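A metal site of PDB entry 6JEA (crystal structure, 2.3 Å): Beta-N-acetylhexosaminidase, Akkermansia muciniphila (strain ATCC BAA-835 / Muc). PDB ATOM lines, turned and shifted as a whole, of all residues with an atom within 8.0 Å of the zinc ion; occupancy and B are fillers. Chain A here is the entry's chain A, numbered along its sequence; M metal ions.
Of the 22 residues printed, 4 come within 4 Å of the zinc ion.
SG of Cys 267 is bound to the zinc ion (2.4 Å).
SG of Cys 270 binds the zinc ion.
The zinc ion is bound by SG of Cys 206, at 2.4 Å.
SG of Cys 226 binds the zinc ion (2.4 Å).
The zinc ion has four donor atoms within binding distance.
N of Leu 269 sits close to SG of Cys 267, at 3.5 Å.
The side-chain sulfur of Cys 270 lies close to the side-chain amide nitrogen of Gln 228 (3.4 Å).
The side-chain amide nitrogen of Gln 285 sits close to the side-chain sulfur of Cys 270 (3.1 Å).
The side-chain sulfur of Cys 226 lies close to the backbone NH of Gln 228, at 3.6 Å.
The backbone NH (N) of Cys 226 sits at hydrogen-bond distance from the backbone carbonyl oxygen (O) of Phe 204 (2.9 Å).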
ATOM      1  N   PHE A 204      -4.861  31.419 -22.165  1.00  0.00           N
ATOM      2  CA  PHE A 204      -4.299  30.118 -21.802  1.00  0.00           C
ATOM      3  C   PHE A 204      -5.045  29.452 -20.654  1.00  0.00           C
ATOM      4  O   PHE A 204      -4.741  28.295 -20.330  1.00  0.00           O
ATOM      5  CB  PHE A 204      -2.824  30.253 -21.392  1.00  0.00           C
ATOM      6  CG  PHE A 204      -1.887  30.605 -22.519  1.00  0.00           C
ATOM      7  CD1 PHE A 204      -2.336  30.670 -23.821  1.00  0.00           C
ATOM      8  CD2 PHE A 204      -0.552  30.864 -22.258  1.00  0.00           C
ATOM      9  CE1 PHE A 204      -1.472  30.999 -24.852  1.00  0.00           C
ATOM     10  CE2 PHE A 204       0.324  31.183 -23.280  1.00  0.00           C
ATOM     11  CZ  PHE A 204      -0.137  31.256 -24.582  1.00  0.00           C
ATOM     12  N   PHE A 205      -6.007  30.139 -20.042  1.00  0.00           N
ATOM     13  CA  PHE A 205      -6.567  29.695 -18.773  1.00  0.00           C
ATOM     14  C   PHE A 205      -8.042  29.370 -18.917  1.00  0.00           C
ATOM     15  O   PHE A 205      -8.725  29.827 -19.846  1.00  0.00           O
ATOM     16  CB  PHE A 205      -6.344  30.763 -17.685  1.00  0.00           C
ATOM     17  CG  PHE A 205      -4.892  30.930 -17.312  1.00  0.00           C
ATOM     18  CD1 PHE A 205      -4.016  31.563 -18.176  1.00  0.00           C
ATOM     19  CD2 PHE A 205      -4.413  30.446 -16.111  1.00  0.00           C
ATOM     20  CE1 PHE A 205      -2.680  31.709 -17.841  1.00  0.00           C
ATOM     21  CE2 PHE A 205      -3.077  30.591 -15.767  1.00  0.00           C
ATOM     22  CZ  PHE A 205      -2.211  31.223 -16.631  1.00  0.00           C
ATOM     23  N   CYS A 206      -8.535  28.554 -17.975  1.00  0.00           N
ATOM     24  CA  CYS A 206      -9.929  28.115 -18.032  1.00  0.00           C
ATOM     25  C   CYS A 206     -10.892  29.292 -17.994  1.00  0.00           C
ATOM     26  O   CYS A 206     -11.883  29.313 -18.736  1.00  0.00           O
ATOM     27  CB  CYS A 206     -10.215  27.164 -16.869  1.00  0.00           C
ATOM     28  SG  CYS A 206      -9.194  25.669 -16.841  1.00  0.00           S
ATOM     29  N   PHE A 207     -10.624  30.277 -17.139  1.00  0.00           N
ATOM     30  CA  PHE A 207     -11.482  31.439 -16.968  1.00  0.00           C
ATOM     31  C   PHE A 207     -10.650  32.692 -17.225  1.00  0.00           C
ATOM     32  O   PHE A 207     -10.150  33.330 -16.292  1.00  0.00           O
ATOM     33  CB  PHE A 207     -12.118  31.446 -15.574  1.00  0.00           C
ATOM     34  CG  PHE A 207     -13.031  30.286 -15.336  1.00  0.00           C
ATOM     35  CD1 PHE A 207     -14.355  30.328 -15.764  1.00  0.00           C
ATOM     36  CD2 PHE A 207     -12.574  29.139 -14.721  1.00  0.00           C
ATOM     37  CE1 PHE A 207     -15.197  29.255 -15.561  1.00  0.00           C
ATOM     38  CE2 PHE A 207     -13.414  28.055 -14.509  1.00  0.00           C
ATOM     39  CZ  PHE A 207     -14.732  28.117 -14.934  1.00  0.00           C
ATOM     40  N   LEU A 224      -4.880  28.062 -13.105  1.00  0.00           N
ATOM     41  CA  LEU A 224      -4.167  26.996 -13.794  1.00  0.00           C
ATOM     42  C   LEU A 224      -4.392  27.130 -15.300  1.00  0.00           C
ATOM     43  O   LEU A 224      -5.485  27.502 -15.741  1.00  0.00           O
ATOM     44  CB  LEU A 224      -4.640  25.621 -13.339  1.00  0.00           C
ATOM     45  CG  LEU A 224      -4.740  25.340 -11.836  1.00  0.00           C
ATOM     46  CD1 LEU A 224      -5.077  23.876 -11.622  1.00  0.00           C
ATOM     47  CD2 LEU A 224      -3.445  25.713 -11.135  1.00  0.00           C
ATOM     48  N   VAL A 225      -3.349  26.836 -16.084  1.00  0.00           N
ATOM     49  CA  VAL A 225      -3.530  26.764 -17.528  1.00  0.00           C
ATOM     50  C   VAL A 225      -4.531  25.662 -17.841  1.00  0.00           C
ATOM     51  O   VAL A 225      -4.643  24.656 -17.125  1.00  0.00           O
ATOM     52  CB  VAL A 225      -2.195  26.523 -18.252  1.00  0.00           C
ATOM     53  CG1 VAL A 225      -1.259  27.691 -18.033  1.00  0.00           C
ATOM     54  CG2 VAL A 225      -1.569  25.225 -17.775  1.00  0.00           C
ATOM     55  N   CYS A 226      -5.293  25.854 -18.913  1.00  0.00           N
ATOM     56  CA  CYS A 226      -6.296  24.885 -19.308  1.00  0.00           C
ATOM     57  C   CYS A 226      -5.653  23.827 -20.200  1.00  0.00           C
ATOM     58  O   CYS A 226      -5.229  24.159 -21.319  1.00  0.00           O
ATOM     59  CB  CYS A 226      -7.452  25.553 -20.031  1.00  0.00           C
ATOM     60  SG  CYS A 226      -8.761  24.412 -20.513  1.00  0.00           S
ATOM     61  N   PRO A 227      -5.556  22.574 -19.756  1.00  0.00           N
ATOM     62  CA  PRO A 227      -4.911  21.549 -20.593  1.00  0.00           C
ATOM     63  C   PRO A 227      -5.636  21.248 -21.889  1.00  0.00           C
ATOM     64  O   PRO A 227      -5.075  20.572 -22.748  1.00  0.00           O
ATOM     65  CB  PRO A 227      -4.882  20.311 -19.684  1.00  0.00           C
ATOM     66  CG  PRO A 227      -5.206  20.804 -18.318  1.00  0.00           C
ATOM     67  CD  PRO A 227      -6.051  22.017 -18.492  1.00  0.00           C
ATOM     68  N   GLN A 228      -6.879  21.711 -22.049  1.00  0.00           N
ATOM     69  CA  GLN A 228      -7.641  21.424 -23.264  1.00  0.00           C
ATOM     70  C   GLN A 228      -7.329  22.394 -24.393  1.00  0.00           C
ATOM     71  O   GLN A 228      -7.792  22.176 -25.515  1.00  0.00           O
ATOM     72  CB  GLN A 228      -9.145  21.438 -22.964  1.00  0.00           C
ATOM     73  CG  GLN A 228      -9.545  20.892 -21.604  1.00  0.00           C
ATOM     74  CD  GLN A 228      -8.932  19.535 -21.297  1.00  0.00           C
ATOM     75  OE1 GLN A 228      -8.694  18.719 -22.199  1.00  0.00           O
ATOM     76  NE2 GLN A 228      -8.688  19.273 -20.022  1.00  0.00           N
ATOM     77  N   LYS A 229      -6.582  23.448 -24.126  1.00  0.00           N
ATOM     78  CA  LYS A 229      -6.390  24.451 -25.174  1.00  0.00           C
ATOM     79  C   LYS A 229      -5.091  24.188 -25.923  1.00  0.00           C
ATOM     80  O   LYS A 229      -4.033  24.080 -25.292  1.00  0.00           O
ATOM     81  CB  LYS A 229      -6.374  25.844 -24.561  1.00  0.00           C
ATOM     82  CG  LYS A 229      -7.630  26.134 -23.745  1.00  0.00           C
ATOM     83  CD  LYS A 229      -7.845  27.610 -23.503  1.00  0.00           C
ATOM     84  CE  LYS A 229      -9.179  27.856 -22.808  1.00  0.00           C
ATOM     85  NZ  LYS A 229      -9.497  29.297 -22.645  1.00  0.00           N
ATOM     86  N   LEU A 263     -10.671  25.545 -10.309  1.00  0.00           N
ATOM     87  CA  LEU A 263     -11.031  26.091 -11.617  1.00  0.00           C
ATOM     88  C   LEU A 263     -11.081  24.994 -12.683  1.00  0.00           C
ATOM     89  O   LEU A 263     -11.925  25.048 -13.587  1.00  0.00           O
ATOM     90  CB  LEU A 263     -10.053  27.200 -12.002  1.00  0.00           C
ATOM     91  CG  LEU A 263     -10.079  28.383 -11.037  1.00  0.00           C
ATOM     92  CD1 LEU A 263      -9.333  29.578 -11.610  1.00  0.00           C
ATOM     93  CD2 LEU A 263     -11.522  28.766 -10.690  1.00  0.00           C
ATOM     94  N   TRP A 264     -10.189  24.003 -12.595  1.00  0.00           N
ATOM     95  CA  TRP A 264     -10.311  22.838 -13.471  1.00  0.00           C
ATOM     96  C   TRP A 264     -11.658  22.152 -13.260  1.00  0.00           C
ATOM     97  O   TRP A 264     -12.295  21.726 -14.237  1.00  0.00           O
ATOM     98  CB  TRP A 264      -9.169  21.857 -13.210  1.00  0.00           C
ATOM     99  CG  TRP A 264      -7.907  22.187 -13.943  1.00  0.00           C
ATOM    100  CD1 TRP A 264      -7.649  23.317 -14.675  1.00  0.00           C
ATOM    101  CD2 TRP A 264      -6.728  21.382 -14.019  1.00  0.00           C
ATOM    102  NE1 TRP A 264      -6.380  23.261 -15.193  1.00  0.00           N
ATOM    103  CE2 TRP A 264      -5.794  22.084 -14.810  1.00  0.00           C
ATOM    104  CE3 TRP A 264      -6.363  20.133 -13.493  1.00  0.00           C
ATOM    105  CZ2 TRP A 264      -4.521  21.575 -15.081  1.00  0.00           C
ATOM    106  CZ3 TRP A 264      -5.111  19.633 -13.774  1.00  0.00           C
ATOM    107  CH2 TRP A 264      -4.199  20.351 -14.563  1.00  0.00           C
ATOM    108  N   GLU A 265     -12.098  22.034 -12.009  1.00  0.00           N
ATOM    109  CA  GLU A 265     -13.398  21.427 -11.733  1.00  0.00           C
ATOM    110  C   GLU A 265     -14.515  22.223 -12.385  1.00  0.00           C
ATOM    111  O   GLU A 265     -15.447  21.636 -12.953  1.00  0.00           O
ATOM    112  CB  GLU A 265     -13.611  21.313 -10.221  1.00  0.00           C
ATOM    113  CG  GLU A 265     -14.830  20.484  -9.813  1.00  0.00           C
ATOM    114  CD  GLU A 265     -16.139  21.261  -9.878  1.00  0.00           C
ATOM    115  OE1 GLU A 265     -16.119  22.483  -9.634  1.00  0.00           O
ATOM    116  OE2 GLU A 265     -17.183  20.639 -10.172  1.00  0.00           O
ATOM    117  N   LYS A 266     -14.450  23.559 -12.325  1.00  0.00           N
ATOM    118  CA  LYS A 266     -15.496  24.393 -12.887  1.00  0.00           C
ATOM    119  C   LYS A 266     -15.400  24.554 -14.408  1.00  0.00           C
ATOM    120  O   LYS A 266     -16.379  24.977 -15.029  1.00  0.00           O
ATOM    121  CB  LYS A 266     -15.490  25.780 -12.245  1.00  0.00           C
ATOM    122  CG  LYS A 266     -15.960  25.813 -10.801  1.00  0.00           C
ATOM    123  CD  LYS A 266     -15.934  27.239 -10.264  1.00  0.00           C
ATOM    124  CE  LYS A 266     -16.619  27.338  -8.919  1.00  0.00           C
ATOM    125  NZ  LYS A 266     -15.985  26.443  -7.906  1.00  0.00           N
ATOM    126  N   CYS A 267     -14.264  24.237 -15.009  1.00  0.00           N
ATOM    127  CA  CYS A 267     -14.050  24.531 -16.425  1.00  0.00           C
ATOM    128  C   CYS A 267     -14.880  23.617 -17.320  1.00  0.00           C
ATOM    129  O   CYS A 267     -14.756  22.387 -17.226  1.00  0.00           O
ATOM    130  CB  CYS A 267     -12.567  24.388 -16.775  1.00  0.00           C
ATOM    131  SG  CYS A 267     -12.230  24.518 -18.554  1.00  0.00           S
ATOM    132  N   PRO A 268     -15.718  24.160 -18.212  1.00  0.00           N
ATOM    133  CA  PRO A 268     -16.545  23.281 -19.062  1.00  0.00           C
ATOM    134  C   PRO A 268     -15.722  22.408 -20.001  1.00  0.00           C
ATOM    135  O   PRO A 268     -16.051  21.232 -20.219  1.00  0.00           O
ATOM    136  CB  PRO A 268     -17.438  24.266 -19.819  1.00  0.00           C
ATOM    137  CG  PRO A 268     -16.690  25.568 -19.789  1.00  0.00           C
ATOM    138  CD  PRO A 268     -15.948  25.586 -18.494  1.00  0.00           C
ATOM    139  N   LEU A 269     -14.632  22.963 -20.545  1.00  0.00           N
ATOM    140  CA  LEU A 269     -13.716  22.177 -21.356  1.00  0.00           C
ATOM    141  C   LEU A 269     -13.136  21.020 -20.556  1.00  0.00           C
ATOM    142  O   LEU A 269     -13.203  19.859 -20.985  1.00  0.00           O
ATOM    143  CB  LEU A 269     -12.588  23.063 -21.900  1.00  0.00           C
ATOM    144  CG  LEU A 269     -12.983  24.288 -22.714  1.00  0.00           C
ATOM    145  CD1 LEU A 269     -11.738  25.019 -23.195  1.00  0.00           C
ATOM    146  CD2 LEU A 269     -13.866  23.897 -23.888  1.00  0.00           C
ATOM    147  N   CYS A 270     -12.565  21.318 -19.387  1.00  0.00           N
ATOM    148  CA  CYS A 270     -11.989  20.259 -18.562  1.00  0.00           C
ATOM    149  C   CYS A 270     -13.047  19.303 -18.036  1.00  0.00           C
ATOM    150  O   CYS A 270     -12.768  18.107 -17.891  1.00  0.00           O
ATOM    151  CB  CYS A 270     -11.196  20.874 -17.399  1.00  0.00           C
ATOM    152  SG  CYS A 270      -9.687  21.755 -17.889  1.00  0.00           S
ATOM    153  N   ARG A 271     -14.257  19.788 -17.747  1.00  0.00           N
ATOM    154  CA  ARG A 271     -15.327  18.897 -17.333  1.00  0.00           C
ATOM    155  C   ARG A 271     -15.614  17.849 -18.400  1.00  0.00           C
ATOM    156  O   ARG A 271     -15.604  16.636 -18.115  1.00  0.00           O
ATOM    157  CB  ARG A 271     -16.599  19.699 -17.038  1.00  0.00           C
ATOM    158  CG  ARG A 271     -16.643  20.288 -15.647  1.00  0.00           C
ATOM    159  CD  ARG A 271     -17.935  21.034 -15.412  1.00  0.00           C
ATOM    160  NE  ARG A 271     -18.101  21.379 -14.001  1.00  0.00           N
ATOM    161  CZ  ARG A 271     -19.103  22.122 -13.534  1.00  0.00           C
ATOM    162  NH1 ARG A 271     -20.017  22.605 -14.366  1.00  0.00           N
ATOM    163  NH2 ARG A 271     -19.172  22.396 -12.241  1.00  0.00           N
ATOM    164  N   ALA A 273     -13.721  17.011 -20.822  1.00  0.00           N
ATOM    165  CA  ALA A 273     -12.533  16.225 -21.097  1.00  0.00           C
ATOM    166  C   ALA A 273     -12.356  15.113 -20.072  1.00  0.00           C
ATOM    167  O   ALA A 273     -11.929  13.998 -20.414  1.00  0.00           O
ATOM    168  CB  ALA A 273     -11.295  17.123 -21.119  1.00  0.00           C
ATOM    169  N   ARG A 274     -12.666  15.387 -18.798  1.00  0.00           N
ATOM    170  CA  ARG A 274     -12.629  14.349 -17.788  1.00  0.00           C
ATOM    171  C   ARG A 274     -13.712  13.307 -18.035  1.00  0.00           C
ATOM    172  O   ARG A 274     -13.473  12.106 -17.891  1.00  0.00           O
ATOM    173  CB  ARG A 274     -12.797  14.951 -16.390  1.00  0.00           C
ATOM    174  CG  ARG A 274     -11.630  15.801 -15.936  1.00  0.00           C
ATOM    175  CD  ARG A 274     -11.723  16.094 -14.449  1.00  0.00           C
ATOM    176  NE  ARG A 274     -12.988  16.734 -14.087  1.00  0.00           N
ATOM    177  CZ  ARG A 274     -13.189  18.042 -14.082  1.00  0.00           C
ATOM    178  NH1 ARG A 274     -12.206  18.869 -14.427  1.00  0.00           N
ATOM    179  NH2 ARG A 274     -14.373  18.532 -13.739  1.00  0.00           N
ATOM    180  N   GLN A 285      -6.777  14.177 -13.739  1.00  0.00           N
ATOM    181  CA  GLN A 285      -6.453  15.164 -14.764  1.00  0.00           C
ATOM    182  C   GLN A 285      -5.041  15.720 -14.577  1.00  0.00           C
ATOM    183  O   GLN A 285      -4.328  15.938 -15.550  1.00  0.00           O
ATOM    184  CB  GLN A 285      -7.488  16.283 -14.747  1.00  0.00           C
ATOM    185  CG  GLN A 285      -7.410  17.211 -15.941  1.00  0.00           C
ATOM    186  CD  GLN A 285      -8.382  18.359 -15.857  1.00  0.00           C
ATOM    187  OE1 GLN A 285      -9.385  18.300 -15.135  1.00  0.00           O
ATOM    188  NE2 GLN A 285      -8.097  19.441 -16.586  1.00  0.00           N
HETATM  189 ZN    ZN M   1      -9.915  24.054 -18.425  1.00  0.00          ZN
